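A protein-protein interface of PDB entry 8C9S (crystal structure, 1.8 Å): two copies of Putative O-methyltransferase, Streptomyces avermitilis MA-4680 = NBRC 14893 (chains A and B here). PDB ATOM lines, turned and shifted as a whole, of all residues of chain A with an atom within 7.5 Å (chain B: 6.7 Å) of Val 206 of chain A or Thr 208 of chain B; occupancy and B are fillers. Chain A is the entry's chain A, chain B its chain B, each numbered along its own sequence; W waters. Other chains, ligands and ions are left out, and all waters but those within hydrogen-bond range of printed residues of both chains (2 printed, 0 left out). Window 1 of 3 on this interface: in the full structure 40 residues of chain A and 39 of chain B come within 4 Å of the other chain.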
ATOM      1  N   TRP A   8     -15.681   9.122  -9.838  1.00  0.00           N
ATOM      2  CA  TRP A   8     -14.489   9.138 -10.735  1.00  0.00           C
ATOM      3  C   TRP A   8     -14.896   9.576 -12.150  1.00  0.00           C
ATOM      4  O   TRP A   8     -14.165  10.410 -12.738  1.00  0.00           O
ATOM      5  CB  TRP A   8     -13.746   7.801 -10.753  1.00  0.00           C
ATOM      6  CG  TRP A   8     -13.306   7.289  -9.420  1.00  0.00           C
ATOM      7  CD1 TRP A   8     -13.166   7.972  -8.243  1.00  0.00           C
ATOM      8  CD2 TRP A   8     -12.957   5.933  -9.134  1.00  0.00           C
ATOM      9  NE1 TRP A   8     -12.765   7.117  -7.240  1.00  0.00           N
ATOM     10  CE2 TRP A   8     -12.612   5.865  -7.766  1.00  0.00           C
ATOM     11  CE3 TRP A   8     -12.883   4.771  -9.913  1.00  0.00           C
ATOM     12  CZ2 TRP A   8     -12.229   4.667  -7.160  1.00  0.00           C
ATOM     13  CZ3 TRP A   8     -12.477   3.600  -9.319  1.00  0.00           C
ATOM     14  CH2 TRP A   8     -12.166   3.550  -7.960  1.00  0.00           C
ATOM     15  N   PHE A  15     -12.867  17.477 -15.653  1.00  0.00           N
ATOM     16  CA  PHE A  15     -11.438  17.732 -15.999  1.00  0.00           C
ATOM     17  C   PHE A  15     -11.227  17.666 -17.503  1.00  0.00           C
ATOM     18  O   PHE A  15     -10.510  18.523 -18.052  1.00  0.00           O
ATOM     19  CB  PHE A  15     -10.511  16.704 -15.341  1.00  0.00           C
ATOM     20  CG  PHE A  15     -10.300  16.852 -13.857  1.00  0.00           C
ATOM     21  CD1 PHE A  15     -10.692  17.995 -13.176  1.00  0.00           C
ATOM     22  CD2 PHE A  15      -9.637  15.848 -13.140  1.00  0.00           C
ATOM     23  CE1 PHE A  15     -10.466  18.125 -11.814  1.00  0.00           C
ATOM     24  CE2 PHE A  15      -9.383  16.004 -11.793  1.00  0.00           C
ATOM     25  CZ  PHE A  15      -9.814  17.134 -11.127  1.00  0.00           C
ATOM     26  N   VAL A 166       5.155   3.839 -19.096  1.00  0.00           N
ATOM     27  CA  VAL A 166       4.512   2.508 -19.103  1.00  0.00           C
ATOM     28  C   VAL A 166       3.072   2.650 -18.605  1.00  0.00           C
ATOM     29  O   VAL A 166       2.873   3.126 -17.482  1.00  0.00           O
ATOM     30  CB  VAL A 166       5.328   1.520 -18.263  1.00  0.00           C
ATOM     31  CG1 VAL A 166       4.795   0.113 -18.461  1.00  0.00           C
ATOM     32  CG2 VAL A 166       6.812   1.590 -18.579  1.00  0.00           C
ATOM     33  N   VAL A 169       0.039  -0.146 -14.967  1.00  0.00           N
ATOM     34  CA  VAL A 169       1.053  -0.788 -14.083  1.00  0.00           C
ATOM     35  C   VAL A 169       0.415  -1.259 -12.773  1.00  0.00           C
ATOM     36  O   VAL A 169       1.134  -1.826 -11.964  1.00  0.00           O
ATOM     37  CB  VAL A 169       2.275   0.109 -13.851  1.00  0.00           C
ATOM     38  CG1 VAL A 169       2.968   0.425 -15.180  1.00  0.00           C
ATOM     39  CG2 VAL A 169       1.955   1.374 -13.079  1.00  0.00           C
ATOM     40  N   VAL A 170      -0.897  -1.104 -12.592  1.00  0.00           N
ATOM     41  CA  VAL A 170      -1.562  -1.437 -11.306  1.00  0.00           C
ATOM     42  C   VAL A 170      -2.370  -2.736 -11.442  1.00  0.00           C
ATOM     43  O   VAL A 170      -2.407  -3.490 -10.437  1.00  0.00           O
ATOM     44  CB  VAL A 170      -2.373  -0.223 -10.826  1.00  0.00           C
ATOM     45  CG1 VAL A 170      -3.383  -0.571  -9.744  1.00  0.00           C
ATOM     46  CG2 VAL A 170      -1.414   0.867 -10.381  1.00  0.00           C
ATOM     47  N   THR A 204       9.132   6.873 -11.328  1.00  0.00           N
ATOM     48  CA  THR A 204       8.095   6.817 -10.293  1.00  0.00           C
ATOM     49  C   THR A 204       6.911   6.104 -10.915  1.00  0.00           C
ATOM     50  O   THR A 204       6.901   5.912 -12.157  1.00  0.00           O
ATOM     51  CB  THR A 204       7.757   8.221  -9.785  1.00  0.00           C
ATOM     52  OG1 THR A 204       7.123   8.098  -8.512  1.00  0.00           O
ATOM     53  CG2 THR A 204       6.896   8.957 -10.778  1.00  0.00           C
ATOM     54  N   ALA A 205       5.969   5.708 -10.075  1.00  0.00           N
ATOM     55  CA  ALA A 205       4.684   5.148 -10.534  1.00  0.00           C
ATOM     56  C   ALA A 205       3.575   5.760  -9.686  1.00  0.00           C
ATOM     57  O   ALA A 205       3.821   6.093  -8.475  1.00  0.00           O
ATOM     58  CB  ALA A 205       4.681   3.641 -10.521  1.00  0.00           C
ATOM     59  N   VAL A 206       2.425   5.937 -10.321  1.00  0.00           N
ATOM     60  CA  VAL A 206       1.263   6.615  -9.699  1.00  0.00           C
ATOM     61  C   VAL A 206      -0.008   5.805  -9.948  1.00  0.00           C
ATOM     62  O   VAL A 206      -0.273   5.469 -11.115  1.00  0.00           O
ATOM     63  CB  VAL A 206       1.127   8.044 -10.245  1.00  0.00           C
ATOM     64  CG1 VAL A 206      -0.163   8.684  -9.724  1.00  0.00           C
ATOM     65  CG2 VAL A 206       2.348   8.871  -9.875  1.00  0.00           C
ATOM     66  N   GLN A 207      -0.766   5.558  -8.872  1.00  0.00           N
ATOM     67  CA  GLN A 207      -2.111   4.945  -8.943  1.00  0.00           C
ATOM     68  C   GLN A 207      -3.112   6.027  -9.349  1.00  0.00           C
ATOM     69  O   GLN A 207      -3.125   7.113  -8.727  1.00  0.00           O
ATOM     70  CB  GLN A 207      -2.492   4.290  -7.616  1.00  0.00           C
ATOM     71  CG  GLN A 207      -1.524   3.209  -7.163  1.00  0.00           C
ATOM     72  CD  GLN A 207      -1.962   2.672  -5.821  1.00  0.00           C
ATOM     73  OE1 GLN A 207      -2.986   1.994  -5.705  1.00  0.00           O
ATOM     74  NE2 GLN A 207      -1.212   3.022  -4.791  1.00  0.00           N
ATOM     75  N   THR A 208      -3.914   5.730 -10.353  1.00  0.00           N
ATOM     76  CA  THR A 208      -4.922   6.668 -10.901  1.00  0.00           C
ATOM     77  C   THR A 208      -6.305   6.039 -10.786  1.00  0.00           C
ATOM     78  O   THR A 208      -6.437   4.778 -10.806  1.00  0.00           O
ATOM     79  CB  THR A 208      -4.580   7.076 -12.345  1.00  0.00           C
ATOM     80  OG1 THR A 208      -4.758   5.927 -13.181  1.00  0.00           O
ATOM     81  CG2 THR A 208      -3.161   7.609 -12.491  1.00  0.00           C
ATOM     82  N   VAL A 209      -7.309   6.893 -10.689  1.00  0.00           N
ATOM     83  CA  VAL A 209      -8.714   6.494 -10.948  1.00  0.00           C
ATOM     84  C   VAL A 209      -9.278   7.474 -11.976  1.00  0.00           C
ATOM     85  O   VAL A 209      -8.625   8.465 -12.295  1.00  0.00           O
ATOM     86  CB  VAL A 209      -9.537   6.404  -9.653  1.00  0.00           C
ATOM     87  CG1 VAL A 209      -9.000   5.332  -8.723  1.00  0.00           C
ATOM     88  CG2 VAL A 209      -9.592   7.738  -8.924  1.00  0.00           C
ATOM     89  N   GLY A 210     -10.419   7.139 -12.550  1.00  0.00           N
ATOM     90  CA  GLY A 210     -11.019   7.929 -13.631  1.00  0.00           C
ATOM     91  C   GLY A 210     -12.041   7.097 -14.367  1.00  0.00           C
ATOM     92  O   GLY A 210     -12.442   6.050 -13.820  1.00  0.00           O
ATOM     93  N   TYR A 214      -9.732   1.861 -11.776  1.00  0.00           N
ATOM     94  CA  TYR A 214      -8.539   1.904 -10.908  1.00  0.00           C
ATOM     95  C   TYR A 214      -7.366   1.370 -11.704  1.00  0.00           C
ATOM     96  O   TYR A 214      -7.432   0.164 -12.089  1.00  0.00           O
ATOM     97  CB  TYR A 214      -8.800   1.079  -9.653  1.00  0.00           C
ATOM     98  CG  TYR A 214      -7.602   0.825  -8.782  1.00  0.00           C
ATOM     99  CD1 TYR A 214      -6.772   1.842  -8.337  1.00  0.00           C
ATOM    100  CD2 TYR A 214      -7.330  -0.471  -8.355  1.00  0.00           C
ATOM    101  CE1 TYR A 214      -5.663   1.565  -7.552  1.00  0.00           C
ATOM    102  CE2 TYR A 214      -6.273  -0.749  -7.516  1.00  0.00           C
ATOM    103  CZ  TYR A 214      -5.426   0.267  -7.131  1.00  0.00           C
ATOM    104  OH  TYR A 214      -4.395  -0.057  -6.323  1.00  0.00           O
ATOM    105  N   ASP A 215      -6.334   2.172 -11.955  1.00  0.00           N
ATOM    106  CA  ASP A 215      -5.129   1.641 -12.647  1.00  0.00           C
ATOM    107  C   ASP A 215      -3.956   2.526 -12.251  1.00  0.00           C
ATOM    108  O   ASP A 215      -3.966   2.981 -11.099  1.00  0.00           O
ATOM    109  CB  ASP A 215      -5.376   1.491 -14.151  1.00  0.00           C
ATOM    110  CG  ASP A 215      -4.500   0.435 -14.834  1.00  0.00           C
ATOM    111  OD1 ASP A 215      -3.478  -0.004 -14.249  1.00  0.00           O
ATOM    112  OD2 ASP A 215      -4.842   0.044 -15.935  1.00  0.00           O
ATOM    113  N   GLY A 216      -2.997   2.747 -13.150  1.00  0.00           N
ATOM    114  CA  GLY A 216      -1.816   3.566 -12.873  1.00  0.00           C
ATOM    115  C   GLY A 216      -0.806   3.514 -13.991  1.00  0.00           C
ATOM    116  O   GLY A 216      -0.983   2.717 -14.926  1.00  0.00           O
ATOM    117  N   PHE A 217       0.187   4.391 -13.947  1.00  0.00           N
ATOM    118  CA  PHE A 217       1.245   4.473 -14.987  1.00  0.00           C
ATOM    119  C   PHE A 217       2.609   4.651 -14.306  1.00  0.00           C
ATOM    120  O   PHE A 217       2.660   5.093 -13.142  1.00  0.00           O
ATOM    121  CB  PHE A 217       0.916   5.608 -15.964  1.00  0.00           C
ATOM    122  CG  PHE A 217       1.046   6.982 -15.370  1.00  0.00           C
ATOM    123  CD1 PHE A 217       0.011   7.558 -14.665  1.00  0.00           C
ATOM    124  CD2 PHE A 217       2.244   7.670 -15.454  1.00  0.00           C
ATOM    125  CE1 PHE A 217       0.163   8.802 -14.086  1.00  0.00           C
ATOM    126  CE2 PHE A 217       2.391   8.919 -14.874  1.00  0.00           C
ATOM    127  CZ  PHE A 217       1.353   9.475 -14.181  1.00  0.00           C
ATOM    128  N   ALA A 218       3.679   4.315 -15.022  1.00  0.00           N
ATOM    129  CA  ALA A 218       5.068   4.640 -14.638  1.00  0.00           C
ATOM    130  C   ALA A 218       5.675   5.621 -15.641  1.00  0.00           C
ATOM    131  O   ALA A 218       5.381   5.518 -16.863  1.00  0.00           O
ATOM    132  CB  ALA A 218       5.879   3.374 -14.554  1.00  0.00           C
ATOM    133  N   LEU A 219       6.544   6.492 -15.123  1.00  0.00           N
ATOM    134  CA  LEU A 219       7.326   7.480 -15.888  1.00  0.00           C
ATOM    135  C   LEU A 219       8.760   7.295 -15.444  1.00  0.00           C
ATOM    136  O   LEU A 219       8.996   7.288 -14.200  1.00  0.00           O
ATOM    137  CB  LEU A 219       6.849   8.902 -15.583  1.00  0.00           C
ATOM    138  CG  LEU A 219       7.787  10.022 -16.051  1.00  0.00           C
ATOM    139  CD1 LEU A 219       7.816  10.089 -17.568  1.00  0.00           C
ATOM    140  CD2 LEU A 219       7.370  11.380 -15.504  1.00  0.00           C
ATOM    141  N   TRP B   8      -4.393   0.221  -1.702  1.00  0.00           N
ATOM    142  CA  TRP B   8      -3.707   1.453  -2.141  1.00  0.00           C
ATOM    143  C   TRP B   8      -2.390   1.605  -1.371  1.00  0.00           C
ATOM    144  O   TRP B   8      -1.411   1.985  -2.019  1.00  0.00           O
ATOM    145  CB  TRP B   8      -4.619   2.682  -2.005  1.00  0.00           C
ATOM    146  CG  TRP B   8      -5.871   2.625  -2.812  1.00  0.00           C
ATOM    147  CD1 TRP B   8      -6.180   1.803  -3.861  1.00  0.00           C
ATOM    148  CD2 TRP B   8      -7.026   3.445  -2.590  1.00  0.00           C
ATOM    149  NE1 TRP B   8      -7.432   2.092  -4.336  1.00  0.00           N
ATOM    150  CE2 TRP B   8      -7.983   3.073  -3.553  1.00  0.00           C
ATOM    151  CE3 TRP B   8      -7.318   4.465  -1.672  1.00  0.00           C
ATOM    152  CZ2 TRP B   8      -9.232   3.689  -3.617  1.00  0.00           C
ATOM    153  CZ3 TRP B   8      -8.552   5.078  -1.740  1.00  0.00           C
ATOM    154  CH2 TRP B   8      -9.484   4.696  -2.709  1.00  0.00           C
ATOM    155  N   ASP B  12       1.331   1.398  -3.056  1.00  0.00           N
ATOM    156  CA  ASP B  12       2.225   2.563  -2.876  1.00  0.00           C
ATOM    157  C   ASP B  12       3.506   2.107  -2.178  1.00  0.00           C
ATOM    158  O   ASP B  12       4.554   2.644  -2.504  1.00  0.00           O
ATOM    159  CB  ASP B  12       1.550   3.718  -2.126  1.00  0.00           C
ATOM    160  CG  ASP B  12       1.092   4.876  -3.000  1.00  0.00           C
ATOM    161  OD1 ASP B  12       0.983   4.692  -4.236  1.00  0.00           O
ATOM    162  OD2 ASP B  12       0.839   5.960  -2.433  1.00  0.00           O
ATOM    163  N   PHE B  15       5.616   0.570  -4.931  1.00  0.00           N
ATOM    164  CA  PHE B  15       6.108   1.618  -5.860  1.00  0.00           C
ATOM    165  C   PHE B  15       7.175   2.487  -5.171  1.00  0.00           C
ATOM    166  O   PHE B  15       8.160   2.899  -5.846  1.00  0.00           O
ATOM    167  CB  PHE B  15       4.956   2.506  -6.349  1.00  0.00           C
ATOM    168  CG  PHE B  15       3.963   1.896  -7.301  1.00  0.00           C
ATOM    169  CD1 PHE B  15       4.164   0.661  -7.897  1.00  0.00           C
ATOM    170  CD2 PHE B  15       2.851   2.636  -7.669  1.00  0.00           C
ATOM    171  CE1 PHE B  15       3.240   0.153  -8.788  1.00  0.00           C
ATOM    172  CE2 PHE B  15       1.947   2.131  -8.583  1.00  0.00           C
ATOM    173  CZ  PHE B  15       2.134   0.888  -9.124  1.00  0.00           C
ATOM    174  N   ASN B  46       6.056   8.951  -3.777  1.00  0.00           N
ATOM    175  CA  ASN B  46       5.974   8.725  -5.249  1.00  0.00           C
ATOM    176  C   ASN B  46       5.542  10.028  -5.937  1.00  0.00           C
ATOM    177  O   ASN B  46       5.957  10.250  -7.081  1.00  0.00           O
ATOM    178  CB  ASN B  46       5.085   7.546  -5.625  1.00  0.00           C
ATOM    179  CG  ASN B  46       3.629   7.743  -5.259  1.00  0.00           C
ATOM    180  OD1 ASN B  46       3.302   8.383  -4.246  1.00  0.00           O
ATOM    181  ND2 ASN B  46       2.741   7.241  -6.098  1.00  0.00           N
ATOM    182  N   GLN B  47       4.781  10.883  -5.255  1.00  0.00           N
ATOM    183  CA  GLN B  47       4.384  12.208  -5.794  1.00  0.00           C
ATOM    184  C   GLN B  47       5.577  13.164  -5.714  1.00  0.00           C
ATOM    185  O   GLN B  47       5.787  13.928  -6.658  1.00  0.00           O
ATOM    186  CB  GLN B  47       3.205  12.792  -5.024  1.00  0.00           C
ATOM    187  CG  GLN B  47       1.986  11.899  -4.952  1.00  0.00           C
ATOM    188  CD  GLN B  47       0.934  12.403  -3.991  1.00  0.00           C
ATOM    189  OE1 GLN B  47       1.173  13.253  -3.124  1.00  0.00           O
ATOM    190  NE2 GLN B  47      -0.260  11.877  -4.162  1.00  0.00           N
ATOM    191  N   LEU B  50       7.756  12.275  -8.541  1.00  0.00           N
ATOM    192  CA  LEU B  50       7.195  12.862  -9.774  1.00  0.00           C
ATOM    193  C   LEU B  50       7.575  14.332  -9.896  1.00  0.00           C
ATOM    194  O   LEU B  50       7.969  14.730 -11.001  1.00  0.00           O
ATOM    195  CB  LEU B  50       5.675  12.724  -9.807  1.00  0.00           C
ATOM    196  CG  LEU B  50       5.043  13.224 -11.103  1.00  0.00           C
ATOM    197  CD1 LEU B  50       5.663  12.533 -12.330  1.00  0.00           C
ATOM    198  CD2 LEU B  50       3.543  12.996 -11.039  1.00  0.00           C
ATOM    199  N   ASP B 167      -1.425  20.936  -6.509  1.00  0.00           N
ATOM    200  CA  ASP B 167      -1.771  19.733  -5.713  1.00  0.00           C
ATOM    201  C   ASP B 167      -3.236  19.820  -5.271  1.00  0.00           C
ATOM    202  O   ASP B 167      -3.781  20.951  -5.154  1.00  0.00           O
ATOM    203  CB  ASP B 167      -0.882  19.513  -4.505  1.00  0.00           C
ATOM    204  CG  ASP B 167      -0.842  18.059  -4.032  1.00  0.00           C
ATOM    205  OD1 ASP B 167      -1.287  17.127  -4.801  1.00  0.00           O
ATOM    206  OD2 ASP B 167      -0.366  17.855  -2.902  1.00  0.00           O
ATOM    207  N   VAL B 170      -8.956  17.564  -6.330  1.00  0.00           N
ATOM    208  CA  VAL B 170     -10.167  16.694  -6.429  1.00  0.00           C
ATOM    209  C   VAL B 170     -11.145  17.048  -5.297  1.00  0.00           C
ATOM    210  O   VAL B 170     -12.356  16.988  -5.544  1.00  0.00           O
ATOM    211  CB  VAL B 170      -9.765  15.205  -6.461  1.00  0.00           C
ATOM    212  CG1 VAL B 170     -10.921  14.305  -6.105  1.00  0.00           C
ATOM    213  CG2 VAL B 170      -9.212  14.842  -7.831  1.00  0.00           C
ATOM    214  N   VAL B 206      -5.326  14.810 -13.148  1.00  0.00           N
ATOM    215  CA  VAL B 206      -5.355  13.338 -12.970  1.00  0.00           C
ATOM    216  C   VAL B 206      -5.856  13.057 -11.559  1.00  0.00           C
ATOM    217  O   VAL B 206      -5.335  13.656 -10.593  1.00  0.00           O
ATOM    218  CB  VAL B 206      -3.975  12.724 -13.267  1.00  0.00           C
ATOM    219  CG1 VAL B 206      -3.921  11.245 -12.923  1.00  0.00           C
ATOM    220  CG2 VAL B 206      -3.554  12.966 -14.714  1.00  0.00           C
ATOM    221  N   GLN B 207      -6.840  12.163 -11.450  1.00  0.00           N
ATOM    222  CA  GLN B 207      -7.280  11.617 -10.138  1.00  0.00           C
ATOM    223  C   GLN B 207      -6.307  10.524  -9.698  1.00  0.00           C
ATOM    224  O   GLN B 207      -5.982   9.643 -10.522  1.00  0.00           O
ATOM    225  CB  GLN B 207      -8.700  11.075 -10.223  1.00  0.00           C
ATOM    226  CG  GLN B 207      -9.703  12.138 -10.583  1.00  0.00           C
ATOM    227  CD  GLN B 207     -11.072  11.508 -10.723  1.00  0.00           C
ATOM    228  OE1 GLN B 207     -11.720  11.165  -9.729  1.00  0.00           O
ATOM    229  NE2 GLN B 207     -11.485  11.298 -11.955  1.00  0.00           N
ATOM    230  N   THR B 208      -5.892  10.566  -8.433  1.00  0.00           N
ATOM    231  CA  THR B 208      -4.908   9.631  -7.865  1.00  0.00           C
ATOM    232  C   THR B 208      -5.508   8.944  -6.636  1.00  0.00           C
ATOM    233  O   THR B 208      -6.407   9.508  -5.955  1.00  0.00           O
ATOM    234  CB  THR B 208      -3.591  10.333  -7.515  1.00  0.00           C
ATOM    235  OG1 THR B 208      -3.798  11.217  -6.408  1.00  0.00           O
ATOM    236  CG2 THR B 208      -2.969  11.045  -8.703  1.00  0.00           C
ATOM    237  N   VAL B 209      -4.988   7.764  -6.354  1.00  0.00           N
ATOM    238  CA  VAL B 209      -5.157   7.100  -5.045  1.00  0.00           C
ATOM    239  C   VAL B 209      -3.763   6.678  -4.577  1.00  0.00           C
ATOM    240  O   VAL B 209      -2.784   6.778  -5.345  1.00  0.00           O
ATOM    241  CB  VAL B 209      -6.197   5.955  -5.098  1.00  0.00           C
ATOM    242  CG1 VAL B 209      -7.581   6.507  -5.414  1.00  0.00           C
ATOM    243  CG2 VAL B 209      -5.841   4.853  -6.077  1.00  0.00           C
ATOM    244  N   GLY B 210      -3.681   6.270  -3.337  1.00  0.00           N
ATOM    245  CA  GLY B 210      -2.430   5.833  -2.703  1.00  0.00           C
ATOM    246  C   GLY B 210      -2.509   6.027  -1.223  1.00  0.00           C
ATOM    247  O   GLY B 210      -3.639   6.014  -0.710  1.00  0.00           O
ATOM    248  N   GLY B 213      -4.931   8.479   0.197  1.00  0.00           N
ATOM    249  CA  GLY B 213      -6.320   8.264  -0.226  1.00  0.00           C
ATOM    250  C   GLY B 213      -6.626   8.925  -1.551  1.00  0.00           C
ATOM    251  O   GLY B 213      -5.688   9.193  -2.339  1.00  0.00           O
ATOM    252  N   TYR B 214      -7.913   9.163  -1.806  1.00  0.00           N
ATOM    253  CA  TYR B 214      -8.436   9.666  -3.099  1.00  0.00           C
ATOM    254  C   TYR B 214      -8.164  11.166  -3.229  1.00  0.00           C
ATOM    255  O   TYR B 214      -8.594  11.956  -2.343  1.00  0.00           O
ATOM    256  CB  TYR B 214      -9.925   9.339  -3.188  1.00  0.00           C
ATOM    257  CG  TYR B 214     -10.648   9.978  -4.342  1.00  0.00           C
ATOM    258  CD1 TYR B 214     -10.230   9.795  -5.650  1.00  0.00           C
ATOM    259  CD2 TYR B 214     -11.785  10.735  -4.119  1.00  0.00           C
ATOM    260  CE1 TYR B 214     -10.931  10.344  -6.709  1.00  0.00           C
ATOM    261  CE2 TYR B 214     -12.492  11.291  -5.172  1.00  0.00           C
ATOM    262  CZ  TYR B 214     -12.063  11.106  -6.471  1.00  0.00           C
ATOM    263  OH  TYR B 214     -12.765  11.659  -7.507  1.00  0.00           O
ATOM    264  N   ASP B 215      -7.429  11.571  -4.266  1.00  0.00           N
ATOM    265  CA  ASP B 215      -7.133  13.006  -4.520  1.00  0.00           C
ATOM    266  C   ASP B 215      -6.764  13.201  -5.994  1.00  0.00           C
ATOM    267  O   ASP B 215      -7.194  12.399  -6.857  1.00  0.00           O
ATOM    268  CB  ASP B 215      -6.044  13.547  -3.589  1.00  0.00           C
ATOM    269  CG  ASP B 215      -6.290  14.999  -3.216  1.00  0.00           C
ATOM    270  OD1 ASP B 215      -6.983  15.716  -4.015  1.00  0.00           O
ATOM    271  OD2 ASP B 215      -5.911  15.365  -2.102  1.00  0.00           O
ATOM    272  N   GLY B 216      -5.962  14.223  -6.282  1.00  0.00           N
ATOM    273  CA  GLY B 216      -5.468  14.429  -7.651  1.00  0.00           C
ATOM    274  C   GLY B 216      -4.690  15.712  -7.789  1.00  0.00           C
ATOM    275  O   GLY B 216      -4.622  16.503  -6.814  1.00  0.00           O
ATOM    276  N   PHE B 217      -4.082  15.894  -8.948  1.00  0.00           N
ATOM    277  CA  PHE B 217      -3.225  17.069  -9.222  1.00  0.00           C
ATOM    278  C   PHE B 217      -3.486  17.575 -10.634  1.00  0.00           C
ATOM    279  O   PHE B 217      -4.022  16.866 -11.482  1.00  0.00           O
ATOM    280  CB  PHE B 217      -1.746  16.736  -8.995  1.00  0.00           C
ATOM    281  CG  PHE B 217      -1.186  15.751  -9.977  1.00  0.00           C
ATOM    282  CD1 PHE B 217      -1.420  14.392  -9.824  1.00  0.00           C
ATOM    283  CD2 PHE B 217      -0.469  16.196 -11.084  1.00  0.00           C
ATOM    284  CE1 PHE B 217      -0.932  13.488 -10.755  1.00  0.00           C
ATOM    285  CE2 PHE B 217       0.001  15.294 -12.017  1.00  0.00           C
ATOM    286  CZ  PHE B 217      -0.231  13.941 -11.853  1.00  0.00           C
HETATM  287  O   HOH W   1      -0.066   6.381  -6.120  1.00  0.00           O
HETATM  288  O   HOH W   2      -8.113  10.838 -13.738  1.00  0.00           O
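The backbone carbonyl oxygen (O) of Trp 8 of chain A lies within hydrogen-bond range of the side-chain amide nitrogen (NE2) of Gln 207 of chain B, 2.9 Å away. OG1 of Thr 204 of chain A lies within hydrogen-bond range of O of Asn 46 of chain B, at 2.8 Å. The side-chain amide nitrogen of Asn 46 of chain B lies within hydrogen-bond range of the backbone carbonyl oxygen of Ala 205 of chain A (2.9 Å). The side-chain amide nitrogen of Gln 207 of chain A is in hydrogen-bond range of the backbone carbonyl oxygen of Trp 8 of chain B (3.0 Å). The side-chain amide nitrogen (NE2) of Gln 207 of chain A sits at hydrogen-bond distance from the side-chain carboxylate (OD1) of Asp 12 of chain B. O of Gln 207 of chain A is in hydrogen-bond range of N of Val 209 of chain B (3.1 Å). The backbone NH (N) of Val 209 of chain A sits at hydrogen-bond distance from the backbone carbonyl oxygen (O) of Gln 207 of chain B (3.1 Å).
OD1 of Asp 215 of chain A lies within hydrogen-bond range of N of Val 170 of chain A (3.3 Å). The backbone carbonyl oxygen of Leu 219 of chain A is in hydrogen-bond range of the backbone NH of Thr 204 of chain A (2.9 Å). The backbone NH of Val 206 of chain A sits at hydrogen-bond distance from the backbone carbonyl oxygen of Phe 217 of chain A (3.0 Å). The side-chain hydroxyl of Tyr 214 of chain A is in hydrogen-bond range of the side-chain amide oxygen of Gln 207 of chain A (2.6 Å). The side-chain amide oxygen (OE1) of Gln 207 of chain B lies within hydrogen-bond range of the side-chain hydroxyl (OH) of Tyr 214 of chain B (2.5 Å).
Among the printed residues, pairs that only touch across the chains: Trp 8 of chain A with Tyr 214 of chain B, Val 169 of chain A with Phe 15 of chain B, Val 170 of chain A with Phe 15 of chain B, Ala 205 of chain A with Phe 15 of chain B, Val 206 of chain A with Asn 46 of chain B, Val 206 of chain A with Thr 208 of chain B, Gln 207 of chain A with Phe 15 of chain B, Gln 207 of chain A with Thr 208 of chain B, Gln 207 of chain A with Gly 210 of chain B, Thr 208 of chain A with Val 206 of chain B, Thr 208 of chain A with Gln 207 of chain B, Val 209 of chain A with Val 209 of chain B, Val 209 of chain A with Tyr 214 of chain B, Gly 210 of chain A with Gln 207 of chain B, Tyr 214 of chain A with Trp 8 of chain B, Tyr 214 of chain A with Val 209 of chain B and Leu 219 of chain A with Leu 50 of chain B.
Val 166 of chain A touches none of the printed residues of chain B. Printed residues of chain B within 4 Å of Val 170 of chain A: Phe 15. Printed residues of chain B within 4 Å of Thr 204 of chain A: Asn 46. Of the printed residues of chain B, Val 209 of chain A touches Gln 207, Val 209 and Tyr 214. Printed residues of chain A within 4 Å of Leu 50 of chain B: Leu 219. Thr 208 of chain B touches just these residues of chain A: Val 206 and Gln 207. Gly 213 of chain B touches none of the printed residues of chain A. The nearest residue of chain B that does not touch Val 206 of chain A is Phe 15 of chain B (4.2 Å). The nearest residue of chain A that does not touch Thr 208 of chain B is Thr 208 of chain A (4.2 Å).
Hydrophobic or aromatic side chains of chain B that line the printed part of chain A: Trp 8, Phe 15, Leu 50, Val 206, Val 209 and Tyr 214. Of the 18 printed residues of chain A, 12 touch a printed residue of chain B. Printed residues of chain A that touch a printed residue of chain B: Trp 8, Val 169, Val 170, Thr 204, Ala 205, Val 206, Gln 207, Thr 208, Val 209, Gly 210, Tyr 214 and Leu 219. Hydrophobic or aromatic side chains of chain A that line the printed part of chain B: Trp 8, Val 169, Val 170, Ala 205, Val 206, Val 209, Tyr 214 and Leu 219. Among the printed residues, 24 pairs touch across the chains.
Trp 8 of chain A touches Tyr 214 of chain B, and with the chains exchanged Tyr 214 of chain A touches Trp 8 of chain B. Gln 207 of chain A touches Thr 208 of chain B, and with the chains exchanged Thr 208 of chain A touches Gln 207 of chain B. Val 209 of chain A touches its own counterpart, Val 209 of chain B. Positions printed for both chains: 8, 15, 170, 206, 207, 208, 209, 210, 214, 215, 216 and 217. Of the 24 pairs that touch across the chains among the printed residues, 15 have their exchanged pair printed and touching as well.
Water W1 lies within hydrogen-bond range of OD1 of Asp 12 of chain B (2.7 Å), O of Val 209 of chain B (2.9 Å), ND2 of Asn 46 of chain B (2.9 Å) and N of Gln 207 of chain A (3.0 Å). Water W2 lies within hydrogen-bond range of O of Val 209 of chain A (2.8 Å) and N of Gln 207 of chain B (2.9 Å).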
